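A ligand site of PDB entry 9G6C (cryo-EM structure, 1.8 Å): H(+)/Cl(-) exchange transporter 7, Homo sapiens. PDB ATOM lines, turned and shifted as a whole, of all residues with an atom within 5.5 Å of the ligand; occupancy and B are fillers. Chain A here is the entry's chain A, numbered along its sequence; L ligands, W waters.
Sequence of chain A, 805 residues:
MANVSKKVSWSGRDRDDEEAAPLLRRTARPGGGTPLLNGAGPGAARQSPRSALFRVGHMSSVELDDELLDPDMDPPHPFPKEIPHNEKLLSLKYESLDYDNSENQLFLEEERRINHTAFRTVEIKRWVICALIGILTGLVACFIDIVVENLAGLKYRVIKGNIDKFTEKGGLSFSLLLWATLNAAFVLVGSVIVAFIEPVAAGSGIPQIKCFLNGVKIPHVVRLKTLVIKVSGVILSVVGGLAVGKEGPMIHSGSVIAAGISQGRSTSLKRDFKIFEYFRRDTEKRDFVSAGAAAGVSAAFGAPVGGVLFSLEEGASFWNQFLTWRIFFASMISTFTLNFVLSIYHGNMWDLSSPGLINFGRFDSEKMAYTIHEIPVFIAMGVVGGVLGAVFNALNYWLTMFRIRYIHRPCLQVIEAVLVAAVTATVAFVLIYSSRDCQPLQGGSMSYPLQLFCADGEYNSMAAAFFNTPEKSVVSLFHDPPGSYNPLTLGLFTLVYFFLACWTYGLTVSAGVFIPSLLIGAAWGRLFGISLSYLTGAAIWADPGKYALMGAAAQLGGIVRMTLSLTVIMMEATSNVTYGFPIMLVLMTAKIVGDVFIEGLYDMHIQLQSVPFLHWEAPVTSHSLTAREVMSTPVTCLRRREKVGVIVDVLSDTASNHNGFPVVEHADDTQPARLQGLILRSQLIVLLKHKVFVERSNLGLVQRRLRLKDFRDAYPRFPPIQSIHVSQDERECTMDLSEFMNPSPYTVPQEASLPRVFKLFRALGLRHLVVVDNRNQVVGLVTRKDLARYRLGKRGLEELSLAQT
Merely in contact with the ligand: Gln 263 (3.2 Å), Leu 227 (3.3 Å), Val 222 (3.3 Å), Gly 260 (3.4 Å), Ile 261 (3.4 Å), Ile 275 (3.5 Å), Gly 264 (3.5 Å), Phe 273 (3.5 Å), Val 140 (3.7 Å), Val 256 (3.8 Å), Phe 276 (3.8 Å), Leu 136 (3.8 Å), Leu 132 (3.9 Å) and Pro 716 (3.96 Å).
Hydrophobic or aromatic side chains that line the ligand: Leu 132, Leu 136, Val 140, Val 222, Leu 224, Leu 227, Val 256, Ile 261, Phe 273, Ile 275, Phe 276 and Pro 716.
Of the 31 residues printed, 23 come within 4 Å of the ligand.
The nearest printed residue that does not touch the ligand is Ile 257 (4.03 Å).
Water W1 lies within hydrogen-bond range of O9 of the ligand (2.7 Å), NZ of Lys 285 (2.7 Å) and OE1 of Gln 263 (2.7 Å).
Water W4 bridges an oxygen (O19) of the ligand and the backbone NH (N) of His 220.
The backbone carbonyl oxygen of Gln 263 sits at hydrogen-bond distance from the guanidinium group of Arg 280, at 3.0 Å.
N of Leu 269 is in hydrogen-bond range of OG of Ser 266, at 3.3 Å.
The backbone carbonyl oxygen (O) of Phe 273 sits at hydrogen-bond distance from the guanidinium group (NH2) of Arg 280 (3.5 Å).
NH1 of Arg 223 lies close to ND1 of His 220, at 3.5 Å.
O of Gly 264 sits at hydrogen-bond distance from N of Phe 273, at 3.2 Å.
The backbone NH (N) of Ser 268 is in hydrogen-bond range of an oxygen (O14) of the ligand, 2.7 Å away.
OG of Ser 268 lies within hydrogen-bond range of O13 of the ligand (2.6 Å).
An oxygen (O9) of the ligand lies within salt-bridge range of the guanidinium group (NE) of Arg 265 (2.6 Å).
The side-chain amino group (NZ) of Lys 285 sits at hydrogen-bond distance from an oxygen (O5) of the ligand, 2.9 Å away.
The side-chain hydroxyl (OG) of Ser 266 lies within hydrogen-bond range of an oxygen (O14) of the ligand (2.8 Å).
The backbone carbonyl oxygen (O) of Arg 265 sits close to an oxygen (O8) of the ligand (3.0 Å).
The guanidinium group (NE) of Arg 223 lies within salt-bridge range of an oxygen (O19) of the ligand (3.0 Å).
An oxygen (O18) of the ligand lies within salt-bridge range of the guanidinium group (NE) of Arg 717, at 3.3 Å.
An oxygen (O5) of the ligand is in hydrogen-bond range of the backbone carbonyl oxygen (O) of Ala 259 (2.9 Å).
The backbone NH (N) of Thr 267 is in hydrogen-bond range of an oxygen (O7) of the ligand.
The side-chain hydroxyl (OG1) of Thr 267 is in hydrogen-bond range of an oxygen (O7) of the ligand.
O13 of the ligand sits at hydrogen-bond distance from N of Leu 224, at 2.7 Å.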
ATOM      1  N   LEU A 132     -28.077 -18.739  21.794  1.00  0.00           N
ATOM      2  CA  LEU A 132     -27.844 -18.857  20.351  1.00  0.00           C
ATOM      3  C   LEU A 132     -26.599 -18.095  19.935  1.00  0.00           C
ATOM      4  O   LEU A 132     -25.853 -18.544  19.054  1.00  0.00           O
ATOM      5  CB  LEU A 132     -29.070 -18.365  19.573  1.00  0.00           C
ATOM      6  CG  LEU A 132     -30.292 -19.282  19.612  1.00  0.00           C
ATOM      7  CD1 LEU A 132     -31.427 -18.701  18.782  1.00  0.00           C
ATOM      8  CD2 LEU A 132     -29.926 -20.676  19.118  1.00  0.00           C
ATOM      9  N   LEU A 136     -23.617 -20.093  18.032  1.00  0.00           N
ATOM     10  CA  LEU A 136     -23.197 -19.716  16.692  1.00  0.00           C
ATOM     11  C   LEU A 136     -21.781 -19.150  16.682  1.00  0.00           C
ATOM     12  O   LEU A 136     -21.021 -19.392  15.744  1.00  0.00           O
ATOM     13  CB  LEU A 136     -24.187 -18.714  16.103  1.00  0.00           C
ATOM     14  CG  LEU A 136     -25.581 -19.287  15.843  1.00  0.00           C
ATOM     15  CD1 LEU A 136     -26.549 -18.193  15.416  1.00  0.00           C
ATOM     16  CD2 LEU A 136     -25.533 -20.395  14.817  1.00  0.00           C
ATOM     17  N   LEU A 139     -19.579 -22.112  16.859  1.00  0.00           N
ATOM     18  CA  LEU A 139     -19.578 -22.837  15.592  1.00  0.00           C
ATOM     19  C   LEU A 139     -18.744 -22.113  14.535  1.00  0.00           C
ATOM     20  O   LEU A 139     -18.070 -22.746  13.727  1.00  0.00           O
ATOM     21  CB  LEU A 139     -21.009 -23.044  15.090  1.00  0.00           C
ATOM     22  CG  LEU A 139     -21.853 -24.072  15.844  1.00  0.00           C
ATOM     23  CD1 LEU A 139     -23.276 -24.088  15.319  1.00  0.00           C
ATOM     24  CD2 LEU A 139     -21.222 -25.453  15.746  1.00  0.00           C
ATOM     25  N   VAL A 140     -18.800 -20.772  14.536  1.00  0.00           N
ATOM     26  CA  VAL A 140     -17.968 -20.004  13.612  1.00  0.00           C
ATOM     27  C   VAL A 140     -16.496 -20.236  13.912  1.00  0.00           C
ATOM     28  O   VAL A 140     -15.675 -20.407  12.996  1.00  0.00           O
ATOM     29  CB  VAL A 140     -18.334 -18.512  13.678  1.00  0.00           C
ATOM     30  CG1 VAL A 140     -17.256 -17.659  13.026  1.00  0.00           C
ATOM     31  CG2 VAL A 140     -19.670 -18.274  12.996  1.00  0.00           C
ATOM     32  N   LYS A 217     -21.123   4.293  16.297  1.00  0.00           N
ATOM     33  CA  LYS A 217     -21.331   3.324  15.221  1.00  0.00           C
ATOM     34  C   LYS A 217     -20.397   3.620  14.058  1.00  0.00           C
ATOM     35  O   LYS A 217     -20.485   4.684  13.439  1.00  0.00           O
ATOM     36  CB  LYS A 217     -22.786   3.359  14.747  1.00  0.00           C
ATOM     37  CG  LYS A 217     -23.779   2.739  15.706  1.00  0.00           C
ATOM     38  CD  LYS A 217     -25.164   2.690  15.083  1.00  0.00           C
ATOM     39  CE  LYS A 217     -25.621   4.066  14.645  1.00  0.00           C
ATOM     40  NZ  LYS A 217     -27.014   4.046  14.102  1.00  0.00           N
ATOM     41  N   HIS A 220     -21.308  -0.208   8.717  1.00  0.00           N
ATOM     42  CA  HIS A 220     -21.178  -1.567   8.173  1.00  0.00           C
ATOM     43  C   HIS A 220     -20.469  -2.532   9.108  1.00  0.00           C
ATOM     44  O   HIS A 220     -19.956  -3.558   8.662  1.00  0.00           O
ATOM     45  CB  HIS A 220     -20.476  -1.545   6.808  1.00  0.00           C
ATOM     46  CG  HIS A 220     -21.142  -0.680   5.783  1.00  0.00           C
ATOM     47  ND1 HIS A 220     -22.363  -0.074   6.005  1.00  0.00           N
ATOM     48  CD2 HIS A 220     -20.760  -0.316   4.544  1.00  0.00           C
ATOM     49  CE1 HIS A 220     -22.698   0.629   4.931  1.00  0.00           C
ATOM     50  NE2 HIS A 220     -21.746   0.500   4.030  1.00  0.00           N
ATOM     51  N   VAL A 221     -20.406  -2.235  10.414  1.00  0.00           N
ATOM     52  CA  VAL A 221     -19.706  -3.136  11.332  1.00  0.00           C
ATOM     53  C   VAL A 221     -20.478  -4.439  11.524  1.00  0.00           C
ATOM     54  O   VAL A 221     -19.883  -5.517  11.586  1.00  0.00           O
ATOM     55  CB  VAL A 221     -19.458  -2.438  12.688  1.00  0.00           C
ATOM     56  CG1 VAL A 221     -18.263  -1.513  12.589  1.00  0.00           C
ATOM     57  CG2 VAL A 221     -20.701  -1.709  13.163  1.00  0.00           C
ATOM     58  N   VAL A 222     -21.808  -4.361  11.608  1.00  0.00           N
ATOM     59  CA  VAL A 222     -22.600  -5.516  12.005  1.00  0.00           C
ATOM     60  C   VAL A 222     -23.497  -5.964  10.865  1.00  0.00           C
ATOM     61  O   VAL A 222     -24.587  -6.502  11.080  1.00  0.00           O
ATOM     62  CB  VAL A 222     -23.430  -5.205  13.270  1.00  0.00           C
ATOM     63  CG1 VAL A 222     -22.523  -5.136  14.490  1.00  0.00           C
ATOM     64  CG2 VAL A 222     -24.197  -3.913  13.091  1.00  0.00           C
ATOM     65  N   ARG A 223     -23.041  -5.755   9.635  1.00  0.00           N
ATOM     66  CA  ARG A 223     -23.755  -6.221   8.461  1.00  0.00           C
ATOM     67  C   ARG A 223     -23.364  -7.660   8.152  1.00  0.00           C
ATOM     68  O   ARG A 223     -22.272  -8.120   8.486  1.00  0.00           O
ATOM     69  CB  ARG A 223     -23.466  -5.331   7.253  1.00  0.00           C
ATOM     70  CG  ARG A 223     -23.928  -3.897   7.436  1.00  0.00           C
ATOM     71  CD  ARG A 223     -24.587  -3.362   6.180  1.00  0.00           C
ATOM     72  NE  ARG A 223     -25.242  -2.080   6.401  1.00  0.00           N
ATOM     73  CZ  ARG A 223     -25.430  -1.164   5.468  1.00  0.00           C
ATOM     74  NH1 ARG A 223     -25.036  -1.351   4.220  1.00  0.00           N
ATOM     75  NH2 ARG A 223     -26.036  -0.028   5.797  1.00  0.00           N
ATOM     76  N   LEU A 224     -24.282  -8.385   7.491  1.00  0.00           N
ATOM     77  CA  LEU A 224     -24.030  -9.778   7.154  1.00  0.00           C
ATOM     78  C   LEU A 224     -22.847  -9.919   6.211  1.00  0.00           C
ATOM     79  O   LEU A 224     -22.033 -10.844   6.354  1.00  0.00           O
ATOM     80  CB  LEU A 224     -25.286 -10.403   6.557  1.00  0.00           C
ATOM     81  CG  LEU A 224     -25.125 -11.788   5.928  1.00  0.00           C
ATOM     82  CD1 LEU A 224     -24.684 -12.811   6.965  1.00  0.00           C
ATOM     83  CD2 LEU A 224     -26.416 -12.234   5.265  1.00  0.00           C
ATOM     84  N   LYS A 225     -22.733  -9.020   5.232  1.00  0.00           N
ATOM     85  CA  LYS A 225     -21.608  -9.079   4.296  1.00  0.00           C
ATOM     86  C   LYS A 225     -20.284  -8.905   5.024  1.00  0.00           C
ATOM     87  O   LYS A 225     -19.286  -9.538   4.654  1.00  0.00           O
ATOM     88  CB  LYS A 225     -21.782  -8.013   3.215  1.00  0.00           C
ATOM     89  CG  LYS A 225     -20.610  -7.903   2.252  1.00  0.00           C
ATOM     90  CD  LYS A 225     -20.620  -6.581   1.518  1.00  0.00           C
ATOM     91  CE  LYS A 225     -21.626  -6.593   0.377  1.00  0.00           C
ATOM     92  NZ  LYS A 225     -21.649  -5.303  -0.362  1.00  0.00           N
ATOM     93  N   LEU A 227     -19.549  -9.899   8.067  1.00  0.00           N
ATOM     94  CA  LEU A 227     -19.220 -11.158   8.728  1.00  0.00           C
ATOM     95  C   LEU A 227     -18.676 -12.169   7.730  1.00  0.00           C
ATOM     96  O   LEU A 227     -17.697 -12.870   8.010  1.00  0.00           O
ATOM     97  CB  LEU A 227     -20.457 -11.722   9.438  1.00  0.00           C
ATOM     98  CG  LEU A 227     -20.337 -13.149   9.968  1.00  0.00           C
ATOM     99  CD1 LEU A 227     -19.284 -13.224  11.050  1.00  0.00           C
ATOM    100  CD2 LEU A 227     -21.672 -13.641  10.491  1.00  0.00           C
ATOM    101  N   VAL A 256     -21.250  -9.454  15.184  1.00  0.00           N
ATOM    102  CA  VAL A 256     -22.170  -9.415  14.045  1.00  0.00           C
ATOM    103  C   VAL A 256     -23.277 -10.429  14.219  1.00  0.00           C
ATOM    104  O   VAL A 256     -24.455 -10.149  13.928  1.00  0.00           O
ATOM    105  CB  VAL A 256     -21.405  -9.625  12.723  1.00  0.00           C
ATOM    106  CG1 VAL A 256     -22.356  -9.511  11.551  1.00  0.00           C
ATOM    107  CG2 VAL A 256     -20.277  -8.623  12.601  1.00  0.00           C
ATOM    108  N   ILE A 257     -22.936 -11.630  14.679  1.00  0.00           N
ATOM    109  CA  ILE A 257     -23.962 -12.644  14.951  1.00  0.00           C
ATOM    110  C   ILE A 257     -24.922 -12.150  16.022  1.00  0.00           C
ATOM    111  O   ILE A 257     -26.147 -12.309  15.904  1.00  0.00           O
ATOM    112  CB  ILE A 257     -23.298 -13.977  15.356  1.00  0.00           C
ATOM    113  CG1 ILE A 257     -22.533 -14.574  14.184  1.00  0.00           C
ATOM    114  CG2 ILE A 257     -24.341 -14.958  15.872  1.00  0.00           C
ATOM    115  CD1 ILE A 257     -21.369 -15.434  14.603  1.00  0.00           C
ATOM    116  N   ALA A 259     -25.671  -9.023  16.840  1.00  0.00           N
ATOM    117  CA  ALA A 259     -26.479  -7.902  16.365  1.00  0.00           C
ATOM    118  C   ALA A 259     -27.492  -8.292  15.301  1.00  0.00           C
ATOM    119  O   ALA A 259     -28.399  -7.513  15.009  1.00  0.00           O
ATOM    120  CB  ALA A 259     -25.573  -6.793  15.815  1.00  0.00           C
ATOM    121  N   GLY A 260     -27.367  -9.490  14.714  1.00  0.00           N
ATOM    122  CA  GLY A 260     -28.312  -9.910  13.692  1.00  0.00           C
ATOM    123  C   GLY A 260     -29.291 -10.957  14.167  1.00  0.00           C
ATOM    124  O   GLY A 260     -30.475 -10.913  13.816  1.00  0.00           O
ATOM    125  N   ILE A 261     -28.807 -11.916  14.957  1.00  0.00           N
ATOM    126  CA  ILE A 261     -29.671 -12.975  15.475  1.00  0.00           C
ATOM    127  C   ILE A 261     -30.717 -12.392  16.422  1.00  0.00           C
ATOM    128  O   ILE A 261     -31.883 -12.785  16.411  1.00  0.00           O
ATOM    129  CB  ILE A 261     -28.840 -14.074  16.149  1.00  0.00           C
ATOM    130  CG1 ILE A 261     -28.260 -15.028  15.095  1.00  0.00           C
ATOM    131  CG2 ILE A 261     -29.650 -14.842  17.182  1.00  0.00           C
ATOM    132  CD1 ILE A 261     -29.307 -15.899  14.431  1.00  0.00           C
ATOM    133  N   GLN A 263     -32.198  -9.618  16.367  1.00  0.00           N
ATOM    134  CA  GLN A 263     -33.263  -8.903  15.668  1.00  0.00           C
ATOM    135  C   GLN A 263     -34.256  -9.836  15.005  1.00  0.00           C
ATOM    136  O   GLN A 263     -35.343  -9.384  14.621  1.00  0.00           O
ATOM    137  CB  GLN A 263     -32.664  -7.959  14.629  1.00  0.00           C
ATOM    138  CG  GLN A 263     -31.523  -7.098  15.140  1.00  0.00           C
ATOM    139  CD  GLN A 263     -31.935  -6.186  16.276  1.00  0.00           C
ATOM    140  OE1 GLN A 263     -32.469  -5.103  16.051  1.00  0.00           O
ATOM    141  NE2 GLN A 263     -31.691  -6.619  17.508  1.00  0.00           N
ATOM    142  N   GLY A 264     -33.926 -11.116  14.861  1.00  0.00           N
ATOM    143  CA  GLY A 264     -34.836 -12.057  14.223  1.00  0.00           C
ATOM    144  C   GLY A 264     -35.139 -11.750  12.778  1.00  0.00           C
ATOM    145  O   GLY A 264     -36.226 -12.066  12.298  1.00  0.00           O
ATOM    146  N   ARG A 265     -34.190 -11.149  12.062  1.00  0.00           N
ATOM    147  CA  ARG A 265     -34.406 -10.767  10.672  1.00  0.00           C
ATOM    148  C   ARG A 265     -33.053 -10.530  10.018  1.00  0.00           C
ATOM    149  O   ARG A 265     -32.030 -10.408  10.693  1.00  0.00           O
ATOM    150  CB  ARG A 265     -35.273  -9.513  10.568  1.00  0.00           C
ATOM    151  CG  ARG A 265     -34.584  -8.246  11.042  1.00  0.00           C
ATOM    152  CD  ARG A 265     -35.400  -7.004  10.715  1.00  0.00           C
ATOM    153  NE  ARG A 265     -34.836  -5.815  11.344  1.00  0.00           N
ATOM    154  CZ  ARG A 265     -35.491  -4.670  11.466  1.00  0.00           C
ATOM    155  NH1 ARG A 265     -36.730  -4.518  11.025  1.00  0.00           N
ATOM    156  NH2 ARG A 265     -34.884  -3.641  12.064  1.00  0.00           N
ATOM    157  N   SER A 266     -33.059 -10.467   8.697  1.00  0.00           N
ATOM    158  CA  SER A 266     -31.869 -10.151   7.908  1.00  0.00           C
ATOM    159  C   SER A 266     -32.210  -9.047   6.929  1.00  0.00           C
ATOM    160  O   SER A 266     -32.927  -9.273   5.942  1.00  0.00           O
ATOM    161  CB  SER A 266     -31.349 -11.391   7.177  1.00  0.00           C
ATOM    162  OG  SER A 266     -30.208 -11.081   6.409  1.00  0.00           O
ATOM    163  N   THR A 267     -31.703  -7.840   7.194  1.00  0.00           N
ATOM    164  CA  THR A 267     -31.941  -6.721   6.280  1.00  0.00           C
ATOM    165  C   THR A 267     -31.242  -6.958   4.947  1.00  0.00           C
ATOM    166  O   THR A 267     -31.811  -6.652   3.889  1.00  0.00           O
ATOM    167  CB  THR A 267     -31.456  -5.416   6.917  1.00  0.00           C
ATOM    168  OG1 THR A 267     -32.217  -5.155   8.108  1.00  0.00           O
ATOM    169  CG2 THR A 267     -31.627  -4.256   5.960  1.00  0.00           C
ATOM    170  N   SER A 268     -30.017  -7.496   4.969  1.00  0.00           N
ATOM    171  CA  SER A 268     -29.283  -7.726   3.734  1.00  0.00           C
ATOM    172  C   SER A 268     -29.979  -8.733   2.840  1.00  0.00           C
ATOM    173  O   SER A 268     -30.052  -8.548   1.615  1.00  0.00           O
ATOM    174  CB  SER A 268     -27.858  -8.196   4.062  1.00  0.00           C
ATOM    175  OG  SER A 268     -27.132  -7.203   4.759  1.00  0.00           O
ATOM    176  N   LEU A 269     -30.524  -9.802   3.422  1.00  0.00           N
ATOM    177  CA  LEU A 269     -31.209 -10.829   2.663  1.00  0.00           C
ATOM    178  C   LEU A 269     -32.696 -10.538   2.474  1.00  0.00           C
ATOM    179  O   LEU A 269     -33.386 -11.324   1.817  1.00  0.00           O
ATOM    180  CB  LEU A 269     -31.044 -12.197   3.341  1.00  0.00           C
ATOM    181  CG  LEU A 269     -29.612 -12.673   3.569  1.00  0.00           C
ATOM    182  CD1 LEU A 269     -29.595 -14.082   4.144  1.00  0.00           C
ATOM    183  CD2 LEU A 269     -28.812 -12.606   2.286  1.00  0.00           C
ATOM    184  N   PHE A 273     -38.102 -12.763   9.789  1.00  0.00           N
ATOM    185  CA  PHE A 273     -38.794 -13.737  10.626  1.00  0.00           C
ATOM    186  C   PHE A 273     -39.544 -13.003  11.727  1.00  0.00           C
ATOM    187  O   PHE A 273     -38.985 -12.143  12.403  1.00  0.00           O
ATOM    188  CB  PHE A 273     -37.792 -14.732  11.218  1.00  0.00           C
ATOM    189  CG  PHE A 273     -36.726 -15.175  10.259  1.00  0.00           C
ATOM    190  CD1 PHE A 273     -36.990 -16.134   9.313  1.00  0.00           C
ATOM    191  CD2 PHE A 273     -35.463 -14.608  10.306  1.00  0.00           C
ATOM    192  CE1 PHE A 273     -36.010 -16.537   8.418  1.00  0.00           C
ATOM    193  CE2 PHE A 273     -34.478 -15.008   9.419  1.00  0.00           C
ATOM    194  CZ  PHE A 273     -34.749 -15.970   8.479  1.00  0.00           C
ATOM    195  N   ILE A 275     -40.196 -12.762  14.652  1.00  0.00           N
ATOM    196  CA  ILE A 275     -39.761 -13.024  16.012  1.00  0.00           C
ATOM    197  C   ILE A 275     -38.776 -11.941  16.430  1.00  0.00           C
ATOM    198  O   ILE A 275     -38.146 -11.284  15.597  1.00  0.00           O
ATOM    199  CB  ILE A 275     -39.118 -14.425  16.171  1.00  0.00           C
ATOM    200  CG1 ILE A 275     -37.902 -14.558  15.256  1.00  0.00           C
ATOM    201  CG2 ILE A 275     -40.135 -15.530  15.904  1.00  0.00           C
ATOM    202  CD1 ILE A 275     -36.780 -15.376  15.845  1.00  0.00           C
ATOM    203  N   PHE A 276     -38.655 -11.762  17.754  1.00  0.00           N
ATOM    204  CA  PHE A 276     -37.658 -10.872  18.356  1.00  0.00           C
ATOM    205  C   PHE A 276     -37.834  -9.421  17.913  1.00  0.00           C
ATOM    206  O   PHE A 276     -36.865  -8.655  17.876  1.00  0.00           O
ATOM    207  CB  PHE A 276     -36.235 -11.346  18.059  1.00  0.00           C
ATOM    208  CG  PHE A 276     -35.922 -12.728  18.577  1.00  0.00           C
ATOM    209  CD1 PHE A 276     -36.710 -13.318  19.545  1.00  0.00           C
ATOM    210  CD2 PHE A 276     -34.832 -13.420  18.085  1.00  0.00           C
ATOM    211  CE1 PHE A 276     -36.422 -14.586  20.014  1.00  0.00           C
ATOM    212  CE2 PHE A 276     -34.539 -14.697  18.553  1.00  0.00           C
ATOM    213  CZ  PHE A 276     -35.341 -15.273  19.514  1.00  0.00           C
ATOM    214  N   ARG A 280     -35.586  -4.921  18.670  1.00  0.00           N
ATOM    215  CA  ARG A 280     -35.100  -4.089  17.569  1.00  0.00           C
ATOM    216  C   ARG A 280     -34.950  -2.644  18.045  1.00  0.00           C
ATOM    217  O   ARG A 280     -35.676  -1.732  17.654  1.00  0.00           O
ATOM    218  CB  ARG A 280     -36.030  -4.195  16.364  1.00  0.00           C
ATOM    219  CG  ARG A 280     -36.059  -5.589  15.759  1.00  0.00           C
ATOM    220  CD  ARG A 280     -37.131  -5.724  14.689  1.00  0.00           C
ATOM    221  NE  ARG A 280     -37.264  -7.113  14.257  1.00  0.00           N
ATOM    222  CZ  ARG A 280     -38.170  -7.536  13.383  1.00  0.00           C
ATOM    223  NH1 ARG A 280     -39.039  -6.707  12.829  1.00  0.00           N
ATOM    224  NH2 ARG A 280     -38.204  -8.833  13.066  1.00  0.00           N
ATOM    225  N   LYS A 285     -29.633  -4.063  21.384  1.00  0.00           N
ATOM    226  CA  LYS A 285     -28.603  -4.493  20.443  1.00  0.00           C
ATOM    227  C   LYS A 285     -27.207  -4.367  21.032  1.00  0.00           C
ATOM    228  O   LYS A 285     -26.372  -5.276  20.885  1.00  0.00           O
ATOM    229  CB  LYS A 285     -28.708  -3.697  19.143  1.00  0.00           C
ATOM    230  CG  LYS A 285     -27.685  -4.106  18.089  1.00  0.00           C
ATOM    231  CD  LYS A 285     -27.898  -3.351  16.785  1.00  0.00           C
ATOM    232  CE  LYS A 285     -29.234  -3.731  16.151  1.00  0.00           C
ATOM    233  NZ  LYS A 285     -29.487  -2.943  14.909  1.00  0.00           N
ATOM    234  N   PRO A 716     -33.205  -0.200  11.866  1.00  0.00           N
ATOM    235  CA  PRO A 716     -32.298   0.895  12.217  1.00  0.00           C
ATOM    236  C   PRO A 716     -32.034   1.874  11.079  1.00  0.00           C
ATOM    237  O   PRO A 716     -31.292   2.828  11.251  1.00  0.00           O
ATOM    238  CB  PRO A 716     -31.024   0.136  12.618  1.00  0.00           C
ATOM    239  CG  PRO A 716     -31.011  -1.053  11.680  1.00  0.00           C
ATOM    240  CD  PRO A 716     -32.449  -1.348  11.313  1.00  0.00           C
ATOM    241  N   ARG A 717     -32.627   1.655   9.902  1.00  0.00           N
ATOM    242  CA  ARG A 717     -32.377   2.522   8.751  1.00  0.00           C
ATOM    243  C   ARG A 717     -33.578   3.449   8.577  1.00  0.00           C
ATOM    244  O   ARG A 717     -34.516   3.180   7.828  1.00  0.00           O
ATOM    245  CB  ARG A 717     -32.114   1.673   7.500  1.00  0.00           C
ATOM    246  CG  ARG A 717     -30.757   1.004   7.498  1.00  0.00           C
ATOM    247  CD  ARG A 717     -30.600   0.056   6.324  1.00  0.00           C
ATOM    248  NE  ARG A 717     -29.598  -0.969   6.583  1.00  0.00           N
ATOM    249  CZ  ARG A 717     -29.146  -1.826   5.672  1.00  0.00           C
ATOM    250  NH1 ARG A 717     -29.605  -1.813   4.428  1.00  0.00           N
ATOM    251  NH2 ARG A 717     -28.226  -2.715   6.020  1.00  0.00           N
HETATM  252  C1  LIG L   1     -32.194 -15.286  12.428  1.00  0.00           C
HETATM  253  C2  LIG L   1     -32.001 -13.847  11.969  1.00  0.00           C
HETATM  254  C3  LIG L   1     -31.306 -13.760  10.610  1.00  0.00           C
HETATM  255  C4  LIG L   1     -29.920 -13.131  10.695  1.00  0.00           C
HETATM  256  C5  LIG L   1     -28.082 -12.132   9.593  1.00  0.00           C
HETATM  257  C6  LIG L   1     -28.236  -9.693  10.138  1.00  0.00           C
HETATM  258  C7  LIG L   1     -27.500  -3.509  10.092  1.00  0.00           C
HETATM  259  C8  LIG L   1     -27.881  -5.061  12.084  1.00  0.00           C
HETATM  260  C9  LIG L   1     -25.595 -12.179  10.759  1.00  0.00           C
HETATM  261  C10 LIG L   1     -26.220 -15.867  11.141  1.00  0.00           C
HETATM  262  C11 LIG L   1     -25.591 -17.086  11.811  1.00  0.00           C
HETATM  263  C12 LIG L   1     -24.139 -17.296  11.415  1.00  0.00           C
HETATM  264  C13 LIG L   1     -23.058 -19.502  12.043  1.00  0.00           C
HETATM  265  C14 LIG L   1     -32.355 -17.510  15.137  1.00  0.00           C
HETATM  266  O1  LIG L   1     -29.231 -13.363  11.640  1.00  0.00           O
HETATM  267  C15 LIG L   1     -33.516 -16.577  15.427  1.00  0.00           C
HETATM  268  C16 LIG L   1     -28.033  -6.001   9.771  1.00  0.00           C
HETATM  269  C17 LIG L   1     -28.100  -4.587   9.175  1.00  0.00           C
HETATM  270  C18 LIG L   1     -27.994  -3.629  11.547  1.00  0.00           C
HETATM  271  C19 LIG L   1     -28.636  -6.034  11.177  1.00  0.00           C
HETATM  272  C20 LIG L   1     -26.071 -13.362  11.597  1.00  0.00           C
HETATM  273  C21 LIG L   1     -25.314 -14.640  11.225  1.00  0.00           C
HETATM  274  C22 LIG L   1     -33.433 -15.268  14.641  1.00  0.00           C
HETATM  275  C23 LIG L   1     -23.845 -18.733  10.993  1.00  0.00           C
HETATM  276  C24 LIG L   1     -33.539 -15.483  13.136  1.00  0.00           C
HETATM  277  C25 LIG L   1     -27.679 -11.045  10.592  1.00  0.00           C
HETATM  278  O2  LIG L   1     -29.472 -12.300   9.667  1.00  0.00           O
HETATM  279  O3  LIG L   1     -26.839  -0.403  11.049  1.00  0.00           O
HETATM  280  O4  LIG L   1     -27.240  -2.784  12.377  1.00  0.00           O
HETATM  281  O5  LIG L   1     -28.431  -5.119  13.380  1.00  0.00           O
HETATM  282  O6  LIG L   1     -29.967  -5.593  11.096  1.00  0.00           O
HETATM  283  O7  LIG L   1     -31.701  -6.993   9.792  1.00  0.00           O
HETATM  284  O8  LIG L   1     -30.705  -7.956  11.828  1.00  0.00           O
HETATM  285  O9  LIG L   1     -32.316  -6.102  11.996  1.00  0.00           O
HETATM  286  O10 LIG L   1     -26.295 -10.966  10.738  1.00  0.00           O
HETATM  287  O11 LIG L   1     -24.609 -12.279  10.109  1.00  0.00           O
HETATM  288  O12 LIG L   1     -27.372  -9.162   9.168  1.00  0.00           O
HETATM  289  O13 LIG L   1     -26.828  -7.411   7.361  1.00  0.00           O
HETATM  290  O14 LIG L   1     -28.916  -8.713   7.151  1.00  0.00           O
HETATM  291  O15 LIG L   1     -28.774  -6.874   8.955  1.00  0.00           O
HETATM  292  O16 LIG L   1     -27.422  -4.571   7.950  1.00  0.00           O
HETATM  293  O17 LIG L   1     -27.884  -2.263   9.580  1.00  0.00           O
HETATM  294  O18 LIG L   1     -27.289   0.076   8.676  1.00  0.00           O
HETATM  295  O19 LIG L   1     -25.448  -1.444   9.303  1.00  0.00           O
HETATM  296  P1  LIG L   1     -27.967  -8.045   8.120  1.00  0.00           P
HETATM  297  P2  LIG L   1     -26.844  -0.979   9.659  1.00  0.00           P
HETATM  298  P3  LIG L   1     -31.191  -6.687  11.175  1.00  0.00           P
HETATM  299  O   HOH W   1     -31.593  -4.123  13.648  1.00  0.00           O
HETATM  300  O   HOH W   2     -25.902  -0.933  14.430  1.00  0.00           O
HETATM  301  O   HOH W   3     -24.353   0.018  12.812  1.00  0.00           O
HETATM  302  O   HOH W   4     -24.042   0.813   8.809  1.00  0.00           O
